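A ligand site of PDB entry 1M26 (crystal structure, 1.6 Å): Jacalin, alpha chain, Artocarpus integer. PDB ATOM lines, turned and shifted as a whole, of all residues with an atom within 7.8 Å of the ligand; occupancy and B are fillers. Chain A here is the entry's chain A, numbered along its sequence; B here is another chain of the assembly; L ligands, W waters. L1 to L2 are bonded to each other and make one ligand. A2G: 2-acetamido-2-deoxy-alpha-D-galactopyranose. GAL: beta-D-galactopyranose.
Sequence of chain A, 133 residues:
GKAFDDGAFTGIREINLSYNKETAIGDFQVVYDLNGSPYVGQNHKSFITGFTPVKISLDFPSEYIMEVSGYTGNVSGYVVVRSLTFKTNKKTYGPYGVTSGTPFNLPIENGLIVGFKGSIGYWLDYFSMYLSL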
ATOM      1  N   GLY A   1      30.807   1.326  17.845  1.00  0.00           N
ATOM      2  CA  GLY A   1      30.108   1.639  19.112  1.00  0.00           C
ATOM      3  C   GLY A   1      31.017   2.339  20.099  1.00  0.00           C
ATOM      4  O   GLY A   1      32.179   2.608  19.795  1.00  0.00           O
ATOM      5  N   LYS A   2      30.491   2.654  21.285  1.00  0.00           N
ATOM      6  CA  LYS A   2      31.271   3.328  22.314  1.00  0.00           C
ATOM      7  C   LYS A   2      31.823   2.275  23.282  1.00  0.00           C
ATOM      8  O   LYS A   2      31.061   1.519  23.884  1.00  0.00           O
ATOM      9  CB  LYS A   2      30.395   4.323  23.096  1.00  0.00           C
ATOM     10  CG  LYS A   2      31.127   5.084  24.177  1.00  0.00           C
ATOM     11  CD  LYS A   2      30.220   6.072  24.889  1.00  0.00           C
ATOM     12  CE  LYS A   2      31.012   6.913  25.881  1.00  0.00           C
ATOM     13  NZ  LYS A   2      30.154   7.880  26.615  1.00  0.00           N
ATOM     14  N   ALA A  24      18.738  -7.300  19.109  1.00  0.00           N
ATOM     15  CA  ALA A  24      19.853  -7.722  19.948  1.00  0.00           C
ATOM     16  C   ALA A  24      19.857  -7.121  21.349  1.00  0.00           C
ATOM     17  O   ALA A  24      18.894  -6.473  21.752  1.00  0.00           O
ATOM     18  CB  ALA A  24      21.150  -7.366  19.201  1.00  0.00           C
ATOM     19  N   ILE A  25      20.962  -7.300  22.066  1.00  0.00           N
ATOM     20  CA  ILE A  25      21.079  -6.735  23.402  1.00  0.00           C
ATOM     21  C   ILE A  25      21.364  -5.241  23.278  1.00  0.00           C
ATOM     22  O   ILE A  25      22.113  -4.831  22.397  1.00  0.00           O
ATOM     23  CB  ILE A  25      22.246  -7.391  24.198  1.00  0.00           C
ATOM     24  CG1 ILE A  25      21.976  -8.888  24.400  1.00  0.00           C
ATOM     25  CG2 ILE A  25      22.442  -6.652  25.541  1.00  0.00           C
ATOM     26  CD1 ILE A  25      20.751  -9.203  25.238  1.00  0.00           C
ATOM     27  N   SER A  46      22.571   2.104  24.956  1.00  0.00           N
ATOM     28  CA  SER A  46      22.517   1.959  23.498  1.00  0.00           C
ATOM     29  C   SER A  46      22.314   3.343  22.887  1.00  0.00           C
ATOM     30  O   SER A  46      21.771   4.220  23.549  1.00  0.00           O
ATOM     31  CB  SER A  46      21.334   1.061  23.075  1.00  0.00           C
ATOM     32  OG  SER A  46      20.958   1.289  21.730  1.00  0.00           O
ATOM     33  N   PHE A  47      22.750   3.553  21.646  1.00  0.00           N
ATOM     34  CA  PHE A  47      22.550   4.847  20.988  1.00  0.00           C
ATOM     35  C   PHE A  47      21.073   5.065  20.658  1.00  0.00           C
ATOM     36  O   PHE A  47      20.650   6.195  20.426  1.00  0.00           O
ATOM     37  CB  PHE A  47      23.331   4.933  19.667  1.00  0.00           C
ATOM     38  CG  PHE A  47      24.825   4.880  19.817  1.00  0.00           C
ATOM     39  CD1 PHE A  47      25.448   5.079  21.039  1.00  0.00           C
ATOM     40  CD2 PHE A  47      25.626   4.661  18.690  1.00  0.00           C
ATOM     41  CE1 PHE A  47      26.843   5.062  21.157  1.00  0.00           C
ATOM     42  CE2 PHE A  47      27.018   4.639  18.794  1.00  0.00           C
ATOM     43  CZ  PHE A  47      27.630   4.841  20.026  1.00  0.00           C
ATOM     44  N   ILE A  48      20.301   3.987  20.607  1.00  0.00           N
ATOM     45  CA  ILE A  48      18.882   4.090  20.259  1.00  0.00           C
ATOM     46  C   ILE A  48      17.925   3.609  21.347  1.00  0.00           C
ATOM     47  O   ILE A  48      18.351   3.074  22.357  1.00  0.00           O
ATOM     48  CB  ILE A  48      18.606   3.321  18.948  1.00  0.00           C
ATOM     49  CG1 ILE A  48      18.867   1.825  19.136  1.00  0.00           C
ATOM     50  CG2 ILE A  48      19.483   3.884  17.843  1.00  0.00           C
ATOM     51  CD1 ILE A  48      18.549   0.976  17.903  1.00  0.00           C
ATOM     52  N   VAL A  75      22.913  -8.202  12.360  1.00  0.00           N
ATOM     53  CA  VAL A  75      21.741  -7.348  12.474  1.00  0.00           C
ATOM     54  C   VAL A  75      22.022  -6.085  11.663  1.00  0.00           C
ATOM     55  O   VAL A  75      22.874  -5.284  12.040  1.00  0.00           O
ATOM     56  CB  VAL A  75      21.477  -6.930  13.933  1.00  0.00           C
ATOM     57  CG1 VAL A  75      20.202  -6.109  14.030  1.00  0.00           C
ATOM     58  CG2 VAL A  75      21.405  -8.163  14.825  1.00  0.00           C
ATOM     59  N   SER A  76      21.308  -5.899  10.550  1.00  0.00           N
ATOM     60  CA  SER A  76      21.513  -4.726   9.709  1.00  0.00           C
ATOM     61  C   SER A  76      22.956  -4.632   9.211  1.00  0.00           C
ATOM     62  O   SER A  76      23.463  -3.537   8.944  1.00  0.00           O
ATOM     63  CB  SER A  76      21.179  -3.437  10.486  1.00  0.00           C
ATOM     64  OG  SER A  76      19.787  -3.337  10.751  1.00  0.00           O
ATOM     65  N   GLY A  77      23.621  -5.771   9.082  1.00  0.00           N
ATOM     66  CA  GLY A  77      24.992  -5.764   8.616  1.00  0.00           C
ATOM     67  C   GLY A  77      26.026  -5.677   9.729  1.00  0.00           C
ATOM     68  O   GLY A  77      27.215  -5.861   9.486  1.00  0.00           O
ATOM     69  N   TYR A  78      25.580  -5.368  10.946  1.00  0.00           N
ATOM     70  CA  TYR A  78      26.487  -5.275  12.087  1.00  0.00           C
ATOM     71  C   TYR A  78      26.495  -6.601  12.828  1.00  0.00           C
ATOM     72  O   TYR A  78      25.436  -7.186  13.075  1.00  0.00           O
ATOM     73  CB  TYR A  78      26.030  -4.201  13.076  1.00  0.00           C
ATOM     74  CG  TYR A  78      25.846  -2.820  12.502  1.00  0.00           C
ATOM     75  CD1 TYR A  78      26.942  -2.029  12.162  1.00  0.00           C
ATOM     76  CD2 TYR A  78      24.569  -2.287  12.309  1.00  0.00           C
ATOM     77  CE1 TYR A  78      26.777  -0.744  11.642  1.00  0.00           C
ATOM     78  CE2 TYR A  78      24.388  -1.011  11.797  1.00  0.00           C
ATOM     79  CZ  TYR A  78      25.500  -0.243  11.463  1.00  0.00           C
ATOM     80  OH  TYR A  78      25.324   1.017  10.941  1.00  0.00           O
ATOM     81  N   VAL A  79      27.682  -7.099  13.185  1.00  0.00           N
ATOM     82  CA  VAL A  79      27.753  -8.337  13.951  1.00  0.00           C
ATOM     83  C   VAL A  79      27.738  -7.894  15.412  1.00  0.00           C
ATOM     84  O   VAL A  79      28.586  -7.109  15.837  1.00  0.00           O
ATOM     85  CB  VAL A  79      29.037  -9.141  13.638  1.00  0.00           C
ATOM     86  CG1 VAL A  79      29.180 -10.293  14.626  1.00  0.00           C
ATOM     87  CG2 VAL A  79      28.964  -9.681  12.217  1.00  0.00           C
ATOM     88  N   VAL A  80      26.764  -8.393  16.163  1.00  0.00           N
ATOM     89  CA  VAL A  80      26.600  -8.013  17.552  1.00  0.00           C
ATOM     90  C   VAL A  80      26.195  -9.188  18.417  1.00  0.00           C
ATOM     91  O   VAL A  80      25.931 -10.274  17.911  1.00  0.00           O
ATOM     92  CB  VAL A  80      25.507  -6.925  17.693  1.00  0.00           C
ATOM     93  CG1 VAL A  80      25.912  -5.673  16.944  1.00  0.00           C
ATOM     94  CG2 VAL A  80      24.180  -7.463  17.143  1.00  0.00           C
ATOM     95  N   VAL A  81      26.116  -8.955  19.733  1.00  0.00           N
ATOM     96  CA  VAL A  81      25.703  -9.993  20.665  1.00  0.00           C
ATOM     97  C   VAL A  81      24.177  -9.930  20.693  1.00  0.00           C
ATOM     98  O   VAL A  81      23.595  -8.981  21.204  1.00  0.00           O
ATOM     99  CB  VAL A  81      26.260  -9.717  22.075  1.00  0.00           C
ATOM    100  CG1 VAL A  81      25.833 -10.820  23.031  1.00  0.00           C
ATOM    101  CG2 VAL A  81      27.794  -9.634  22.004  1.00  0.00           C
ATOM    102  N   SER A 119      31.726  -2.960  24.217  1.00  0.00           N
ATOM    103  CA  SER A 119      31.364  -1.825  23.375  1.00  0.00           C
ATOM    104  C   SER A 119      29.887  -1.919  23.010  1.00  0.00           C
ATOM    105  O   SER A 119      29.383  -3.002  22.709  1.00  0.00           O
ATOM    106  CB  SER A 119      32.188  -1.821  22.096  1.00  0.00           C
ATOM    107  OG  SER A 119      31.701  -0.859  21.178  1.00  0.00           O
ATOM    108  N   ILE A 120      29.204  -0.781  23.025  1.00  0.00           N
ATOM    109  CA  ILE A 120      27.789  -0.726  22.682  1.00  0.00           C
ATOM    110  C   ILE A 120      27.543   0.430  21.716  1.00  0.00           C
ATOM    111  O   ILE A 120      27.958   1.561  21.969  1.00  0.00           O
ATOM    112  CB  ILE A 120      26.911  -0.514  23.948  1.00  0.00           C
ATOM    113  CG1 ILE A 120      27.065  -1.707  24.889  1.00  0.00           C
ATOM    114  CG2 ILE A 120      25.440  -0.347  23.544  1.00  0.00           C
ATOM    115  CD1 ILE A 120      26.353  -1.538  26.215  1.00  0.00           C
ATOM    116  N   GLY A 121      26.897   0.135  20.589  1.00  0.00           N
ATOM    117  CA  GLY A 121      26.551   1.157  19.620  1.00  0.00           C
ATOM    118  C   GLY A 121      25.029   1.095  19.638  1.00  0.00           C
ATOM    119  O   GLY A 121      24.417   1.434  20.652  1.00  0.00           O
ATOM    120  N   TYR A 122      24.421   0.659  18.550  1.00  0.00           N
ATOM    121  CA  TYR A 122      22.971   0.498  18.572  1.00  0.00           C
ATOM    122  C   TYR A 122      22.762  -0.681  19.528  1.00  0.00           C
ATOM    123  O   TYR A 122      21.822  -0.712  20.308  1.00  0.00           O
ATOM    124  CB  TYR A 122      22.435   0.088  17.202  1.00  0.00           C
ATOM    125  CG  TYR A 122      22.615   1.097  16.091  1.00  0.00           C
ATOM    126  CD1 TYR A 122      22.767   2.454  16.353  1.00  0.00           C
ATOM    127  CD2 TYR A 122      22.571   0.677  14.769  1.00  0.00           C
ATOM    128  CE1 TYR A 122      22.881   3.371  15.307  1.00  0.00           C
ATOM    129  CE2 TYR A 122      22.674   1.585  13.714  1.00  0.00           C
ATOM    130  CZ  TYR A 122      22.821   2.926  13.999  1.00  0.00           C
ATOM    131  OH  TYR A 122      22.924   3.817  12.951  1.00  0.00           O
ATOM    132  N   TRP A 123      23.670  -1.647  19.431  1.00  0.00           N
ATOM    133  CA  TRP A 123      23.597  -2.859  20.243  1.00  0.00           C
ATOM    134  C   TRP A 123      24.950  -3.211  20.828  1.00  0.00           C
ATOM    135  O   TRP A 123      25.964  -2.601  20.493  1.00  0.00           O
ATOM    136  CB  TRP A 123      23.094  -4.014  19.372  1.00  0.00           C
ATOM    137  CG  TRP A 123      21.800  -3.703  18.680  1.00  0.00           C
ATOM    138  CD1 TRP A 123      20.589  -3.509  19.272  1.00  0.00           C
ATOM    139  CD2 TRP A 123      21.622  -3.447  17.285  1.00  0.00           C
ATOM    140  NE1 TRP A 123      19.655  -3.148  18.323  1.00  0.00           N
ATOM    141  CE2 TRP A 123      20.263  -3.096  17.096  1.00  0.00           C
ATOM    142  CE3 TRP A 123      22.467  -3.471  16.171  1.00  0.00           C
ATOM    143  CZ2 TRP A 123      19.730  -2.776  15.843  1.00  0.00           C
ATOM    144  CZ3 TRP A 123      21.947  -3.150  14.922  1.00  0.00           C
ATOM    145  CH2 TRP A 123      20.587  -2.807  14.770  1.00  0.00           C
ATOM    146  N   LEU A 124      24.956  -4.200  21.728  1.00  0.00           N
ATOM    147  CA  LEU A 124      26.193  -4.667  22.352  1.00  0.00           C
ATOM    148  C   LEU A 124      27.045  -5.292  21.237  1.00  0.00           C
ATOM    149  O   LEU A 124      26.678  -6.332  20.678  1.00  0.00           O
ATOM    150  CB  LEU A 124      25.852  -5.713  23.422  1.00  0.00           C
ATOM    151  CG  LEU A 124      27.007  -6.391  24.168  1.00  0.00           C
ATOM    152  CD1 LEU A 124      27.817  -5.359  24.935  1.00  0.00           C
ATOM    153  CD2 LEU A 124      26.430  -7.432  25.124  1.00  0.00           C
ATOM    154  N   ASP A 125      28.164  -4.658  20.914  1.00  0.00           N
ATOM    155  CA  ASP A 125      29.041  -5.135  19.845  1.00  0.00           C
ATOM    156  C   ASP A 125      29.857  -6.348  20.244  1.00  0.00           C
ATOM    157  O   ASP A 125      30.011  -7.301  19.470  1.00  0.00           O
ATOM    158  CB  ASP A 125      30.002  -4.029  19.420  1.00  0.00           C
ATOM    159  CG  ASP A 125      29.279  -2.781  18.944  1.00  0.00           C
ATOM    160  OD1 ASP A 125      28.451  -2.905  18.029  1.00  0.00           O
ATOM    161  OD2 ASP A 125      29.544  -1.698  19.499  1.00  0.00           O
ATOM    162  N   TYR A 126      30.385  -6.301  21.454  1.00  0.00           N
ATOM    163  CA  TYR A 126      31.182  -7.391  21.985  1.00  0.00           C
ATOM    164  C   TYR A 126      31.433  -7.090  23.438  1.00  0.00           C
ATOM    165  O   TYR A 126      31.162  -5.992  23.914  1.00  0.00           O
ATOM    166  CB  TYR A 126      32.518  -7.482  21.230  1.00  0.00           C
ATOM    167  CG  TYR A 126      33.365  -6.235  21.275  1.00  0.00           C
ATOM    168  CD1 TYR A 126      34.110  -5.913  22.406  1.00  0.00           C
ATOM    169  CD2 TYR A 126      33.387  -5.354  20.203  1.00  0.00           C
ATOM    170  CE1 TYR A 126      34.869  -4.744  22.459  1.00  0.00           C
ATOM    171  CE2 TYR A 126      34.135  -4.180  20.240  1.00  0.00           C
ATOM    172  CZ  TYR A 126      34.875  -3.887  21.378  1.00  0.00           C
ATOM    173  OH  TYR A 126      35.604  -2.728  21.410  1.00  0.00           O
ATOM    174  N   ALA B  14      31.664  -8.951  17.715  1.00  0.00           N
ATOM    175  CA  ALA B  14      32.302  -8.496  16.483  1.00  0.00           C
ATOM    176  C   ALA B  14      33.759  -8.159  16.784  1.00  0.00           C
ATOM    177  O   ALA B  14      34.092  -8.019  17.959  1.00  0.00           O
ATOM    178  CB  ALA B  14      31.892  -7.078  16.358  1.00  0.00           C
ATOM    179  N   LYS B  15      34.638  -8.012  15.809  1.00  0.00           N
ATOM    180  CA  LYS B  15      35.941  -7.754  16.316  1.00  0.00           C
ATOM    181  C   LYS B  15      36.666  -6.473  16.381  1.00  0.00           C
ATOM    182  O   LYS B  15      37.820  -6.639  16.701  1.00  0.00           O
ATOM    183  CB  LYS B  15      36.835  -8.862  15.873  1.00  0.00           C
ATOM    184  CG  LYS B  15      37.011  -9.659  17.091  1.00  0.00           C
ATOM    185  CD  LYS B  15      37.735 -10.839  16.855  1.00  0.00           C
ATOM    186  CE  LYS B  15      37.968 -11.511  18.154  1.00  0.00           C
ATOM    187  NZ  LYS B  15      38.739 -12.755  17.888  1.00  0.00           N
HETATM  188  O5  A2G L   1      25.946   0.639  16.041  1.00  0.00           O
HETATM  189  C1  A2G L   1      26.405   1.900  15.410  1.00  0.00           C
HETATM  190  O1  A2G L   1      25.942   1.950  14.063  1.00  0.00           O
HETATM  191  C2  A2G L   1      27.917   1.973  15.515  1.00  0.00           C
HETATM  192  N2  A2G L   1      28.179   3.222  14.928  1.00  0.00           N
HETATM  193  C3  A2G L   1      28.567   0.732  14.904  1.00  0.00           C
HETATM  194  O3  A2G L   1      29.960   0.863  15.011  1.00  0.00           O
HETATM  195  C4  A2G L   1      28.136  -0.527  15.694  1.00  0.00           C
HETATM  196  O4  A2G L   1      28.510  -0.311  17.070  1.00  0.00           O
HETATM  197  C5  A2G L   1      26.560  -0.640  15.542  1.00  0.00           C
HETATM  198  C6  A2G L   1      25.995  -1.870  16.271  1.00  0.00           C
HETATM  199  O6  A2G L   1      25.992  -1.689  17.680  1.00  0.00           O
HETATM  200  C7  A2G L   1      29.017   4.133  15.481  1.00  0.00           C
HETATM  201  O7  A2G L   1      29.626   3.940  16.550  1.00  0.00           O
HETATM  202  C8  A2G L   1      29.198   5.447  14.757  1.00  0.00           C
HETATM  203  C1  GAL L   2      30.890   0.571  13.934  1.00  0.00           C
HETATM  204  C2  GAL L   2      32.257   1.246  13.987  1.00  0.00           C
HETATM  205  C3  GAL L   2      33.218   0.597  13.015  1.00  0.00           C
HETATM  206  C4  GAL L   2      33.393  -0.943  13.361  1.00  0.00           C
HETATM  207  C5  GAL L   2      31.993  -1.615  13.244  1.00  0.00           C
HETATM  208  C6  GAL L   2      31.619  -3.091  13.436  1.00  0.00           C
HETATM  209  O2  GAL L   2      32.057   2.630  13.716  1.00  0.00           O
HETATM  210  O3  GAL L   2      34.481   1.244  13.104  1.00  0.00           O
HETATM  211  O4  GAL L   2      33.850  -1.128  14.715  1.00  0.00           O
HETATM  212  O5  GAL L   2      31.056  -0.889  14.176  1.00  0.00           O
HETATM  213  O6  GAL L   2      30.427  -3.869  13.365  1.00  0.00           O
HETATM  214  O   HOH W   1      32.711  -0.957  17.985  1.00  0.00           O
HETATM  215  O   HOH W   2      26.014   6.575  14.791  1.00  0.00           O
HETATM  216  O   HOH W   3      26.025   4.530  12.803  1.00  0.00           O
HETATM  217  O   HOH W   4      29.123  -4.360  15.679  1.00  0.00           O
HETATM  218  O   HOH W   5      31.155   5.791  18.668  1.00  0.00           O
HETATM  219  O   HOH W   6      30.266   2.079  10.896  1.00  0.00           O
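O4 of A2G L1 lies within hydrogen-bond range of N of Gly 1 (2.9 Å).
O5 of A2G L1 lies within hydrogen-bond range of N of Tyr 122, at 2.9 Å.
The side-chain hydroxyl (OH) of Tyr 78 sits at hydrogen-bond distance from an oxygen (O1) of A2G L1 (3.3 Å).
An oxygen (O6) of A2G L1 is in hydrogen-bond range of the backbone NH (N) of Trp 123 (2.9 Å).
OD1 of Asp 125 lies within hydrogen-bond range of O6 of A2G L1.
O of Trp 123 lies within hydrogen-bond range of O6 of A2G L1.
Water W4 lies within hydrogen-bond range of an oxygen (O6) of GAL L2, the backbone carbonyl oxygen of Val 79 and the side-chain carboxylate of Asp 125.
Water W3 lies within hydrogen-bond range of an oxygen (O1) of A2G L1 and the side-chain hydroxyl (OH) of Tyr 122.
Water W1 lies within hydrogen-bond range of the backbone NH of Gly 1 (3.0 Å), the side-chain hydroxyl of Ser 119 (3.4 Å) and an oxygen (O4) of GAL L2 (3.5 Å).
Residues that only touch the ligand: Phe 47 (3.5 Å), Val 80 (3.9 Å) and Gly 121 (3.5 Å).
Hydrophobic or aromatic side chains that line the ligand: Phe 47, Tyr 78, Val 80, Tyr 122 and Trp 123.
Of the 24 residues printed, 8 come within 4 Å of the ligand.
The backbone NH of Phe 47 is in hydrogen-bond range of the backbone carbonyl oxygen of Gly 121.
The backbone NH of Asp 125 is in hydrogen-bond range of the backbone carbonyl oxygen of Ser 119 (2.7 Å).
The backbone NH (N) of Ala 14 of chain B lies within hydrogen-bond range of the backbone carbonyl oxygen (O) of Asp 125 (2.9 Å).
O of Tyr 122 sits at hydrogen-bond distance from OG of Ser 46, 2.6 Å away.
The side-chain carboxylate of Asp 125 is in hydrogen-bond range of the backbone NH of Gly 121 (3.4 Å).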
